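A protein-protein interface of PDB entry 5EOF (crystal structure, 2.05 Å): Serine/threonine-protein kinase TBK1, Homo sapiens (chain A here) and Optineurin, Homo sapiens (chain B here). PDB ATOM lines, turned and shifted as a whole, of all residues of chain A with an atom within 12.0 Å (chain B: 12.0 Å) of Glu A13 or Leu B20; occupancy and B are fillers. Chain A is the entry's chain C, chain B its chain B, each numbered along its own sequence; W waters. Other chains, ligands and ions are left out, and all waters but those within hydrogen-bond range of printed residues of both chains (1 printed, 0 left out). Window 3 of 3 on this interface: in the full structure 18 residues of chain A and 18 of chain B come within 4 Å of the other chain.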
ATOM      1  N   PRO A   6      -2.692  19.225 -23.382  1.00  0.00           N
ATOM      2  CA  PRO A   6      -1.731  20.314 -23.577  1.00  0.00           C
ATOM      3  C   PRO A   6      -1.520  20.691 -25.046  1.00  0.00           C
ATOM      4  O   PRO A   6      -0.869  21.703 -25.317  1.00  0.00           O
ATOM      5  CB  PRO A   6      -0.456  19.741 -22.971  1.00  0.00           C
ATOM      6  CG  PRO A   6      -0.966  18.944 -21.839  1.00  0.00           C
ATOM      7  CD  PRO A   6      -2.253  18.312 -22.313  1.00  0.00           C
ATOM      8  N   SER A   7      -2.058  19.894 -25.970  1.00  0.00           N
ATOM      9  CA  SER A   7      -2.081  20.270 -27.383  1.00  0.00           C
ATOM     10  C   SER A   7      -2.957  21.508 -27.572  1.00  0.00           C
ATOM     11  O   SER A   7      -3.802  21.811 -26.724  1.00  0.00           O
ATOM     12  CB  SER A   7      -2.616  19.127 -28.247  1.00  0.00           C
ATOM     13  OG  SER A   7      -1.698  18.053 -28.298  1.00  0.00           O
ATOM     14  N   SER A   8      -2.750  22.222 -28.677  1.00  0.00           N
ATOM     15  CA  SER A   8      -3.548  23.406 -28.976  1.00  0.00           C
ATOM     16  C   SER A   8      -5.044  23.084 -28.934  1.00  0.00           C
ATOM     17  O   SER A   8      -5.802  23.702 -28.181  1.00  0.00           O
ATOM     18  CB  SER A   8      -3.166  23.974 -30.339  1.00  0.00           C
ATOM     19  OG  SER A   8      -3.751  25.244 -30.542  1.00  0.00           O
ATOM     20  N   ASN A   9      -5.459  22.104 -29.732  1.00  0.00           N
ATOM     21  CA  ASN A   9      -6.865  21.728 -29.812  1.00  0.00           C
ATOM     22  C   ASN A   9      -7.479  21.417 -28.445  1.00  0.00           C
ATOM     23  O   ASN A   9      -8.581  21.885 -28.122  1.00  0.00           O
ATOM     24  CB  ASN A   9      -7.053  20.549 -30.767  1.00  0.00           C
ATOM     25  CG  ASN A   9      -8.463  20.002 -30.738  1.00  0.00           C
ATOM     26  OD1 ASN A   9      -9.387  20.614 -31.276  1.00  0.00           O
ATOM     27  ND2 ASN A   9      -8.640  18.847 -30.098  1.00  0.00           N
ATOM     28  N   THR A  10      -6.750  20.643 -27.642  1.00  0.00           N
ATOM     29  CA  THR A  10      -7.206  20.286 -26.304  1.00  0.00           C
ATOM     30  C   THR A  10      -7.421  21.531 -25.438  1.00  0.00           C
ATOM     31  O   THR A  10      -8.463  21.676 -24.818  1.00  0.00           O
ATOM     32  CB  THR A  10      -6.226  19.342 -25.605  1.00  0.00           C
ATOM     33  OG1 THR A  10      -6.009  18.190 -26.429  1.00  0.00           O
ATOM     34  CG2 THR A  10      -6.800  18.902 -24.260  1.00  0.00           C
ATOM     35  N   LEU A  11      -6.436  22.430 -25.426  1.00  0.00           N
ATOM     36  CA  LEU A  11      -6.513  23.651 -24.636  1.00  0.00           C
ATOM     37  C   LEU A  11      -7.623  24.586 -25.114  1.00  0.00           C
ATOM     38  O   LEU A  11      -8.285  25.236 -24.301  1.00  0.00           O
ATOM     39  CB  LEU A  11      -5.159  24.362 -24.634  1.00  0.00           C
ATOM     40  CG  LEU A  11      -4.067  23.628 -23.856  1.00  0.00           C
ATOM     41  CD1 LEU A  11      -2.834  24.479 -23.741  1.00  0.00           C
ATOM     42  CD2 LEU A  11      -4.581  23.290 -22.475  1.00  0.00           C
ATOM     43  N   VAL A  12      -7.835  24.644 -26.427  1.00  0.00           N
ATOM     44  CA  VAL A  12      -8.903  25.468 -26.988  1.00  0.00           C
ATOM     45  C   VAL A  12     -10.265  24.914 -26.574  1.00  0.00           C
ATOM     46  O   VAL A  12     -11.152  25.655 -26.147  1.00  0.00           O
ATOM     47  CB  VAL A  12      -8.809  25.551 -28.528  1.00  0.00           C
ATOM     48  CG1 VAL A  12     -10.079  26.136 -29.118  1.00  0.00           C
ATOM     49  CG2 VAL A  12      -7.598  26.387 -28.944  1.00  0.00           C
ATOM     50  N   GLU A  13     -10.423  23.601 -26.684  1.00  0.00           N
ATOM     51  CA  GLU A  13     -11.695  22.988 -26.345  1.00  0.00           C
ATOM     52  C   GLU A  13     -11.949  23.017 -24.838  1.00  0.00           C
ATOM     53  O   GLU A  13     -13.086  23.215 -24.409  1.00  0.00           O
ATOM     54  CB  GLU A  13     -11.806  21.570 -26.916  1.00  0.00           C
ATOM     55  CG  GLU A  13     -13.233  21.041 -26.923  1.00  0.00           C
ATOM     56  CD  GLU A  13     -13.356  19.667 -27.542  1.00  0.00           C
ATOM     57  OE1 GLU A  13     -14.022  18.800 -26.939  1.00  0.00           O
ATOM     58  OE2 GLU A  13     -12.794  19.457 -28.635  1.00  0.00           O
ATOM     59  N   MET A  14     -10.899  22.843 -24.034  1.00  0.00           N
ATOM     60  CA  MET A  14     -11.044  22.958 -22.577  1.00  0.00           C
ATOM     61  C   MET A  14     -11.378  24.388 -22.181  1.00  0.00           C
ATOM     62  O   MET A  14     -12.169  24.610 -21.271  1.00  0.00           O
ATOM     63  CB  MET A  14      -9.777  22.521 -21.843  1.00  0.00           C
ATOM     64  CG  MET A  14      -9.575  21.018 -21.814  1.00  0.00           C
ATOM     65  SD  MET A  14     -10.875  20.220 -20.865  1.00  0.00           S
ATOM     66  CE  MET A  14     -10.473  20.773 -19.198  1.00  0.00           C
ATOM     67  N   THR A  15     -10.771  25.351 -22.870  1.00  0.00           N
ATOM     68  CA  THR A  15     -10.997  26.762 -22.567  1.00  0.00           C
ATOM     69  C   THR A  15     -12.448  27.144 -22.830  1.00  0.00           C
ATOM     70  O   THR A  15     -13.096  27.738 -21.980  1.00  0.00           O
ATOM     71  CB  THR A  15     -10.072  27.670 -23.391  1.00  0.00           C
ATOM     72  OG1 THR A  15      -8.719  27.417 -23.019  1.00  0.00           O
ATOM     73  CG2 THR A  15     -10.393  29.142 -23.131  1.00  0.00           C
ATOM     74  N   LEU A  16     -12.938  26.797 -24.016  1.00  0.00           N
ATOM     75  CA  LEU A  16     -14.334  26.997 -24.381  1.00  0.00           C
ATOM     76  C   LEU A  16     -15.257  26.378 -23.341  1.00  0.00           C
ATOM     77  O   LEU A  16     -16.196  27.025 -22.868  1.00  0.00           O
ATOM     78  CB  LEU A  16     -14.616  26.353 -25.734  1.00  0.00           C
ATOM     79  CG  LEU A  16     -14.922  27.270 -26.912  1.00  0.00           C
ATOM     80  CD1 LEU A  16     -13.862  28.357 -27.041  1.00  0.00           C
ATOM     81  CD2 LEU A  16     -15.012  26.445 -28.193  1.00  0.00           C
ATOM     82  N   GLY A  17     -14.992  25.124 -22.986  1.00  0.00           N
ATOM     83  CA  GLY A  17     -15.806  24.451 -21.992  1.00  0.00           C
ATOM     84  C   GLY A  17     -15.764  25.138 -20.639  1.00  0.00           C
ATOM     85  O   GLY A  17     -16.797  25.308 -19.985  1.00  0.00           O
ATOM     86  N   MET A  18     -14.575  25.549 -20.217  1.00  0.00           N
ATOM     87  CA  MET A  18     -14.424  26.130 -18.889  1.00  0.00           C
ATOM     88  C   MET A  18     -15.086  27.500 -18.795  1.00  0.00           C
ATOM     89  O   MET A  18     -15.663  27.857 -17.764  1.00  0.00           O
ATOM     90  CB  MET A  18     -12.949  26.232 -18.526  1.00  0.00           C
ATOM     91  CG  MET A  18     -12.720  26.326 -17.038  1.00  0.00           C
ATOM     92  SD  MET A  18     -13.075  24.770 -16.202  1.00  0.00           S
ATOM     93  CE  MET A  18     -11.706  23.782 -16.794  1.00  0.00           C
ATOM     94  N   LYS A  19     -15.011  28.262 -19.879  1.00  0.00           N
ATOM     95  CA  LYS A  19     -15.700  29.543 -19.952  1.00  0.00           C
ATOM     96  C   LYS A  19     -17.217  29.351 -19.931  1.00  0.00           C
ATOM     97  O   LYS A  19     -17.940  30.128 -19.300  1.00  0.00           O
ATOM     98  CB  LYS A  19     -15.248  30.319 -21.188  1.00  0.00           C
ATOM     99  CG  LYS A  19     -13.811  30.802 -21.095  1.00  0.00           C
ATOM    100  CD  LYS A  19     -13.432  31.613 -22.325  1.00  0.00           C
ATOM    101  CE  LYS A  19     -12.076  32.283 -22.173  1.00  0.00           C
ATOM    102  NZ  LYS A  19     -11.728  33.045 -23.404  1.00  0.00           N
ATOM    103  N   LYS A  20     -17.693  28.301 -20.592  1.00  0.00           N
ATOM    104  CA  LYS A  20     -19.122  27.999 -20.597  1.00  0.00           C
ATOM    105  C   LYS A  20     -19.639  27.603 -19.214  1.00  0.00           C
ATOM    106  O   LYS A  20     -20.732  28.010 -18.807  1.00  0.00           O
ATOM    107  CB  LYS A  20     -19.439  26.916 -21.633  1.00  0.00           C
ATOM    108  CG  LYS A  20     -20.904  26.493 -21.672  1.00  0.00           C
ATOM    109  CD  LYS A  20     -21.825  27.668 -21.983  1.00  0.00           C
ATOM    110  CE  LYS A  20     -23.224  27.197 -22.362  1.00  0.00           C
ATOM    111  NZ  LYS A  20     -24.048  28.324 -22.893  1.00  0.00           N
ATOM    112  N   LEU A  21     -18.847  26.824 -18.484  1.00  0.00           N
ATOM    113  CA  LEU A  21     -19.193  26.417 -17.121  1.00  0.00           C
ATOM    114  C   LEU A  21     -19.290  27.629 -16.195  1.00  0.00           C
ATOM    115  O   LEU A  21     -20.145  27.681 -15.322  1.00  0.00           O
ATOM    116  CB  LEU A  21     -18.118  25.469 -16.588  1.00  0.00           C
ATOM    117  CG  LEU A  21     -18.379  23.994 -16.258  1.00  0.00           C
ATOM    118  CD1 LEU A  21     -19.639  23.408 -16.909  1.00  0.00           C
ATOM    119  CD2 LEU A  21     -17.163  23.182 -16.640  1.00  0.00           C
ATOM    120  N   LYS A  22     -18.384  28.583 -16.374  1.00  0.00           N
ATOM    121  CA  LYS A  22     -18.379  29.802 -15.580  1.00  0.00           C
ATOM    122  C   LYS A  22     -19.615  30.639 -15.876  1.00  0.00           C
ATOM    123  O   LYS A  22     -20.204  31.223 -14.973  1.00  0.00           O
ATOM    124  CB  LYS A  22     -17.120  30.615 -15.876  1.00  0.00           C
ATOM    125  CG  LYS A  22     -15.912  30.256 -15.019  1.00  0.00           C
ATOM    126  CD  LYS A  22     -16.119  30.726 -13.577  1.00  0.00           C
ATOM    127  CE  LYS A  22     -14.848  31.324 -12.975  1.00  0.00           C
ATOM    128  NZ  LYS A  22     -13.831  30.292 -12.642  1.00  0.00           N
ATOM    129  N   GLU A  23     -19.991  30.700 -17.150  1.00  0.00           N
ATOM    130  CA  GLU A  23     -21.178  31.432 -17.575  1.00  0.00           C
ATOM    131  C   GLU A  23     -22.440  30.859 -16.941  1.00  0.00           C
ATOM    132  O   GLU A  23     -23.269  31.589 -16.395  1.00  0.00           O
ATOM    133  CB  GLU A  23     -21.324  31.352 -19.091  1.00  0.00           C
ATOM    134  CG  GLU A  23     -20.515  32.349 -19.866  1.00  0.00           C
ATOM    135  CD  GLU A  23     -20.864  32.299 -21.335  1.00  0.00           C
ATOM    136  OE1 GLU A  23     -19.996  32.637 -22.166  1.00  0.00           O
ATOM    137  OE2 GLU A  23     -22.015  31.907 -21.651  1.00  0.00           O
ATOM    138  N   THR B  13      -5.331   8.495 -14.306  1.00  0.00           N
ATOM    139  CA  THR B  13      -4.994   9.793 -14.872  1.00  0.00           C
ATOM    140  C   THR B  13      -5.608   9.915 -16.259  1.00  0.00           C
ATOM    141  O   THR B  13      -5.374   9.065 -17.110  1.00  0.00           O
ATOM    142  CB  THR B  13      -3.474   9.960 -14.965  1.00  0.00           C
ATOM    143  OG1 THR B  13      -2.921   9.990 -13.642  1.00  0.00           O
ATOM    144  CG2 THR B  13      -3.110  11.246 -15.712  1.00  0.00           C
ATOM    145  N   PHE B  14      -6.404  10.957 -16.483  1.00  0.00           N
ATOM    146  CA  PHE B  14      -7.058  11.153 -17.779  1.00  0.00           C
ATOM    147  C   PHE B  14      -6.067  11.341 -18.927  1.00  0.00           C
ATOM    148  O   PHE B  14      -5.075  12.068 -18.796  1.00  0.00           O
ATOM    149  CB  PHE B  14      -7.976  12.384 -17.754  1.00  0.00           C
ATOM    150  CG  PHE B  14      -9.216  12.224 -16.906  1.00  0.00           C
ATOM    151  CD1 PHE B  14      -9.742  10.964 -16.628  1.00  0.00           C
ATOM    152  CD2 PHE B  14      -9.865  13.350 -16.392  1.00  0.00           C
ATOM    153  CE1 PHE B  14     -10.899  10.832 -15.847  1.00  0.00           C
ATOM    154  CE2 PHE B  14     -11.017  13.222 -15.615  1.00  0.00           C
ATOM    155  CZ  PHE B  14     -11.527  11.961 -15.339  1.00  0.00           C
ATOM    156  N   THR B  15      -6.361  10.711 -20.060  1.00  0.00           N
ATOM    157  CA  THR B  15      -5.704  11.061 -21.312  1.00  0.00           C
ATOM    158  C   THR B  15      -6.337  12.367 -21.783  1.00  0.00           C
ATOM    159  O   THR B  15      -7.374  12.783 -21.236  1.00  0.00           O
ATOM    160  CB  THR B  15      -5.908   9.969 -22.380  1.00  0.00           C
ATOM    161  OG1 THR B  15      -7.251  10.024 -22.866  1.00  0.00           O
ATOM    162  CG2 THR B  15      -5.633   8.581 -21.805  1.00  0.00           C
ATOM    163  N   PRO B  16      -5.729  13.025 -22.789  1.00  0.00           N
ATOM    164  CA  PRO B  16      -6.356  14.248 -23.302  1.00  0.00           C
ATOM    165  C   PRO B  16      -7.794  13.982 -23.752  1.00  0.00           C
ATOM    166  O   PRO B  16      -8.687  14.755 -23.394  1.00  0.00           O
ATOM    167  CB  PRO B  16      -5.481  14.604 -24.502  1.00  0.00           C
ATOM    168  CG  PRO B  16      -4.138  14.062 -24.144  1.00  0.00           C
ATOM    169  CD  PRO B  16      -4.412  12.779 -23.412  1.00  0.00           C
ATOM    170  N   GLU B  17      -8.004  12.890 -24.490  1.00  0.00           N
ATOM    171  CA  GLU B  17      -9.331  12.525 -24.986  1.00  0.00           C
ATOM    172  C   GLU B  17     -10.334  12.339 -23.844  1.00  0.00           C
ATOM    173  O   GLU B  17     -11.487  12.785 -23.943  1.00  0.00           O
ATOM    174  CB  GLU B  17      -9.259  11.258 -25.849  1.00  0.00           C
ATOM    175  CG  GLU B  17      -8.548  11.429 -27.188  1.00  0.00           C
ATOM    176  N   GLU B  18      -9.891  11.680 -22.772  1.00  0.00           N
ATOM    177  CA  GLU B  18     -10.732  11.423 -21.608  1.00  0.00           C
ATOM    178  C   GLU B  18     -11.053  12.723 -20.866  1.00  0.00           C
ATOM    179  O   GLU B  18     -12.125  12.876 -20.287  1.00  0.00           O
ATOM    180  CB  GLU B  18     -10.048  10.435 -20.663  1.00  0.00           C
ATOM    181  CG  GLU B  18      -9.929   9.020 -21.232  1.00  0.00           C
ATOM    182  CD  GLU B  18      -9.120   8.093 -20.339  1.00  0.00           C
ATOM    183  OE1 GLU B  18      -9.098   6.870 -20.610  1.00  0.00           O
ATOM    184  OE2 GLU B  18      -8.500   8.586 -19.368  1.00  0.00           O
ATOM    185  N   LEU B  19     -10.109  13.654 -20.904  1.00  0.00           N
ATOM    186  CA  LEU B  19     -10.260  14.933 -20.225  1.00  0.00           C
ATOM    187  C   LEU B  19     -11.339  15.749 -20.923  1.00  0.00           C
ATOM    188  O   LEU B  19     -12.188  16.361 -20.267  1.00  0.00           O
ATOM    189  CB  LEU B  19      -8.915  15.678 -20.213  1.00  0.00           C
ATOM    190  CG  LEU B  19      -8.884  17.016 -19.473  1.00  0.00           C
ATOM    191  CD1 LEU B  19      -9.224  16.845 -17.998  1.00  0.00           C
ATOM    192  CD2 LEU B  19      -7.514  17.679 -19.649  1.00  0.00           C
ATOM    193  N   LEU B  20     -11.314  15.742 -22.254  1.00  0.00           N
ATOM    194  CA  LEU B  20     -12.341  16.415 -23.045  1.00  0.00           C
ATOM    195  C   LEU B  20     -13.713  15.756 -22.886  1.00  0.00           C
ATOM    196  O   LEU B  20     -14.736  16.454 -22.856  1.00  0.00           O
ATOM    197  CB  LEU B  20     -11.959  16.451 -24.524  1.00  0.00           C
ATOM    198  CG  LEU B  20     -10.752  17.302 -24.936  1.00  0.00           C
ATOM    199  CD1 LEU B  20     -10.567  17.297 -26.456  1.00  0.00           C
ATOM    200  CD2 LEU B  20     -10.916  18.706 -24.427  1.00  0.00           C
ATOM    201  N   GLN B  21     -13.745  14.423 -22.816  1.00  0.00           N
ATOM    202  CA  GLN B  21     -15.004  13.714 -22.574  1.00  0.00           C
ATOM    203  C   GLN B  21     -15.595  14.176 -21.263  1.00  0.00           C
ATOM    204  O   GLN B  21     -16.788  14.447 -21.170  1.00  0.00           O
ATOM    205  CB  GLN B  21     -14.786  12.201 -22.495  1.00  0.00           C
ATOM    206  CG  GLN B  21     -15.135  11.429 -23.762  1.00  0.00           C
ATOM    207  CD  GLN B  21     -14.452  10.061 -23.816  1.00  0.00           C
ATOM    208  OE1 GLN B  21     -14.619   9.234 -22.916  1.00  0.00           O
ATOM    209  NE2 GLN B  21     -13.664   9.829 -24.866  1.00  0.00           N
ATOM    210  N   GLN B  22     -14.749  14.239 -20.240  1.00  0.00           N
ATOM    211  CA  GLN B  22     -15.202  14.585 -18.897  1.00  0.00           C
ATOM    212  C   GLN B  22     -15.690  16.024 -18.886  1.00  0.00           C
ATOM    213  O   GLN B  22     -16.643  16.346 -18.190  1.00  0.00           O
ATOM    214  CB  GLN B  22     -14.069  14.380 -17.887  1.00  0.00           C
ATOM    215  CG  GLN B  22     -14.469  14.557 -16.450  1.00  0.00           C
ATOM    216  CD  GLN B  22     -15.641  13.669 -16.060  1.00  0.00           C
ATOM    217  OE1 GLN B  22     -16.672  14.152 -15.571  1.00  0.00           O
ATOM    218  NE2 GLN B  22     -15.495  12.364 -16.282  1.00  0.00           N
ATOM    219  N   MET B  23     -15.047  16.883 -19.678  1.00  0.00           N
ATOM    220  CA  MET B  23     -15.491  18.268 -19.811  1.00  0.00           C
ATOM    221  C   MET B  23     -16.882  18.360 -20.440  1.00  0.00           C
ATOM    222  O   MET B  23     -17.734  19.108 -19.956  1.00  0.00           O
ATOM    223  CB  MET B  23     -14.483  19.101 -20.604  1.00  0.00           C
ATOM    224  CG  MET B  23     -15.005  20.469 -20.981  1.00  0.00           C
ATOM    225  SD  MET B  23     -15.406  21.509 -19.542  1.00  0.00           S
ATOM    226  CE  MET B  23     -13.755  22.027 -19.074  1.00  0.00           C
ATOM    227  N   LYS B  24     -17.118  17.609 -21.516  1.00  0.00           N
ATOM    228  CA  LYS B  24     -18.456  17.564 -22.109  1.00  0.00           C
ATOM    229  C   LYS B  24     -19.519  17.058 -21.132  1.00  0.00           C
ATOM    230  O   LYS B  24     -20.660  17.533 -21.152  1.00  0.00           O
ATOM    231  CB  LYS B  24     -18.468  16.732 -23.394  1.00  0.00           C
ATOM    232  CG  LYS B  24     -17.721  17.395 -24.541  1.00  0.00           C
ATOM    233  CD  LYS B  24     -18.046  16.762 -25.885  1.00  0.00           C
ATOM    234  CE  LYS B  24     -17.670  17.716 -27.014  1.00  0.00           C
ATOM    235  NZ  LYS B  24     -18.285  19.061 -26.793  1.00  0.00           N
ATOM    236  N   GLU B  25     -19.164  16.109 -20.269  1.00  0.00           N
ATOM    237  CA  GLU B  25     -20.137  15.641 -19.276  1.00  0.00           C
ATOM    238  C   GLU B  25     -20.494  16.710 -18.263  1.00  0.00           C
ATOM    239  O   GLU B  25     -21.647  16.804 -17.847  1.00  0.00           O
ATOM    240  CB  GLU B  25     -19.668  14.380 -18.555  1.00  0.00           C
ATOM    241  CG  GLU B  25     -20.757  13.730 -17.695  1.00  0.00           C
ATOM    242  CD  GLU B  25     -20.246  12.546 -16.889  1.00  0.00           C
ATOM    243  OE1 GLU B  25     -19.274  12.723 -16.120  1.00  0.00           O
ATOM    244  OE2 GLU B  25     -20.811  11.437 -17.022  1.00  0.00           O
ATOM    245  N   LEU B  26     -19.504  17.515 -17.881  1.00  0.00           N
ATOM    246  CA  LEU B  26     -19.732  18.595 -16.926  1.00  0.00           C
ATOM    247  C   LEU B  26     -20.651  19.657 -17.502  1.00  0.00           C
ATOM    248  O   LEU B  26     -21.498  20.211 -16.794  1.00  0.00           O
ATOM    249  CB  LEU B  26     -18.411  19.233 -16.502  1.00  0.00           C
ATOM    250  CG  LEU B  26     -17.567  18.379 -15.559  1.00  0.00           C
ATOM    251  CD1 LEU B  26     -16.390  19.192 -15.042  1.00  0.00           C
ATOM    252  CD2 LEU B  26     -18.421  17.857 -14.398  1.00  0.00           C
ATOM    253  N   LEU B  27     -20.468  19.946 -18.786  1.00  0.00           N
ATOM    254  CA  LEU B  27     -21.297  20.919 -19.489  1.00  0.00           C
ATOM    255  C   LEU B  27     -22.729  20.437 -19.486  1.00  0.00           C
ATOM    256  O   LEU B  27     -23.645  21.187 -19.151  1.00  0.00           O
ATOM    257  CB  LEU B  27     -20.806  21.098 -20.930  1.00  0.00           C
ATOM    258  CG  LEU B  27     -19.509  21.888 -20.997  1.00  0.00           C
ATOM    259  CD1 LEU B  27     -18.843  21.797 -22.375  1.00  0.00           C
ATOM    260  CD2 LEU B  27     -19.816  23.304 -20.643  1.00  0.00           C
ATOM    261  N   THR B  28     -22.912  19.171 -19.843  1.00  0.00           N
ATOM    262  CA  THR B  28     -24.234  18.558 -19.851  1.00  0.00           C
ATOM    263  C   THR B  28     -24.887  18.643 -18.474  1.00  0.00           C
ATOM    264  O   THR B  28     -26.031  19.114 -18.336  1.00  0.00           O
ATOM    265  CB  THR B  28     -24.140  17.104 -20.292  1.00  0.00           C
ATOM    266  OG1 THR B  28     -23.854  17.054 -21.697  1.00  0.00           O
ATOM    267  CG2 THR B  28     -25.435  16.382 -20.018  1.00  0.00           C
ATOM    268  N   GLU B  29     -24.158  18.214 -17.448  1.00  0.00           N
ATOM    269  CA  GLU B  29     -24.703  18.223 -16.090  1.00  0.00           C
ATOM    270  C   GLU B  29     -25.023  19.645 -15.609  1.00  0.00           C
ATOM    271  O   GLU B  29     -26.085  19.890 -15.033  1.00  0.00           O
ATOM    272  CB  GLU B  29     -23.734  17.527 -15.127  1.00  0.00           C
ATOM    273  CG  GLU B  29     -23.600  16.013 -15.345  1.00  0.00           C
ATOM    274  CD  GLU B  29     -22.806  15.335 -14.231  1.00  0.00           C
ATOM    275  OE1 GLU B  29     -22.246  16.058 -13.372  1.00  0.00           O
ATOM    276  OE2 GLU B  29     -22.744  14.085 -14.209  1.00  0.00           O
HETATM  277  O   HOH W   1     -14.751  19.212 -24.138  1.00  0.00           O
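Among the printed residues, pairs that only touch across the chains: Thr A10 with Leu B20, Glu A13 with Leu B20, Glu A13 with Lys B24, Met A14 with Leu B20, Met A14 with Met B23, Gly A17 with Met B23, Gly A17 with Leu B27, Met A18 with Met B23, Lys A20 with Leu B27, Leu A21 with Met B23, Leu A21 with Leu B26 and Leu A21 with Leu B27.
Water W1 bridges OE1 of Glu A13 (2.9 Å) and O of Leu B20 (3.0 Å).
Ser A7 touches none of the printed residues of chain B.
Thr A10 touches one residue of chain B.
Leu A11 touches none of the printed residues of chain B.
No residue of chain B comes within 4 Å of Val A12.
Printed residues of chain B within 4 Å of Glu A13: Leu B20 (3.8 Å) and Lys B24 (3.8 Å).
Of chain B, only Leu B20 and Met B23 come within 4 Å of Met A14.
No residue of chain B comes within 4 Å of Thr A15.
No residue of chain B comes within 4 Å of Leu A16.
Of chain B, only Met B23 and Leu B27 come within 4 Å of Gly A17.
Of the printed residues of chain B, Met A18 touches Met B23.
Of the printed residues of chain B, Lys A20 touches Leu B27.
Of the printed residues of chain B, Leu A21 touches Met B23 (3.8 Å), Leu B26 (3.7 Å) and Leu B27 (3.7 Å).
No residue of chain A comes within 4 Å of Pro B16.
No residue of chain A comes within 4 Å of Glu B17.
No residue of chain A comes within 4 Å of Leu B19.
Of the printed residues of chain A, Leu B20 touches Thr A10 (3.9 Å), Glu A13 (3.8 Å) and Met A14 (3.7 Å).
No residue of chain A comes within 4 Å of Gln B21.
Met B23 touches just these residues of chain A: Met A14, Gly A17, Met A18 and Leu A21.
Of chain A, only Glu A13 comes within 4 Å of Lys B24.
Of the printed residues of chain A, Leu B27 touches Gly A17 (3.7 Å), Lys A20 (3.5 Å) and Leu A21 (3.7 Å).
The nearest residue of chain B that does not touch Glu A13 is Met B23 (4.8 Å).
The nearest printed residue of chain B that does not touch Lys A20 is Met B23 (7.1 Å).
Of the 18 printed residues of chain A, 7 touch a printed residue of chain B.
Printed residues of chain A that touch a printed residue of chain B: Thr A10, Glu A13, Met A14, Gly A17, Met A18, Lys A20 and Leu A21.
Among the printed residues, 12 pairs touch across the chains.
The backbone carbonyl oxygen (O) of Lys B24 lies within hydrogen-bond range of the side-chain hydroxyl (OG1) of Thr B28, at 3.3 Å.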
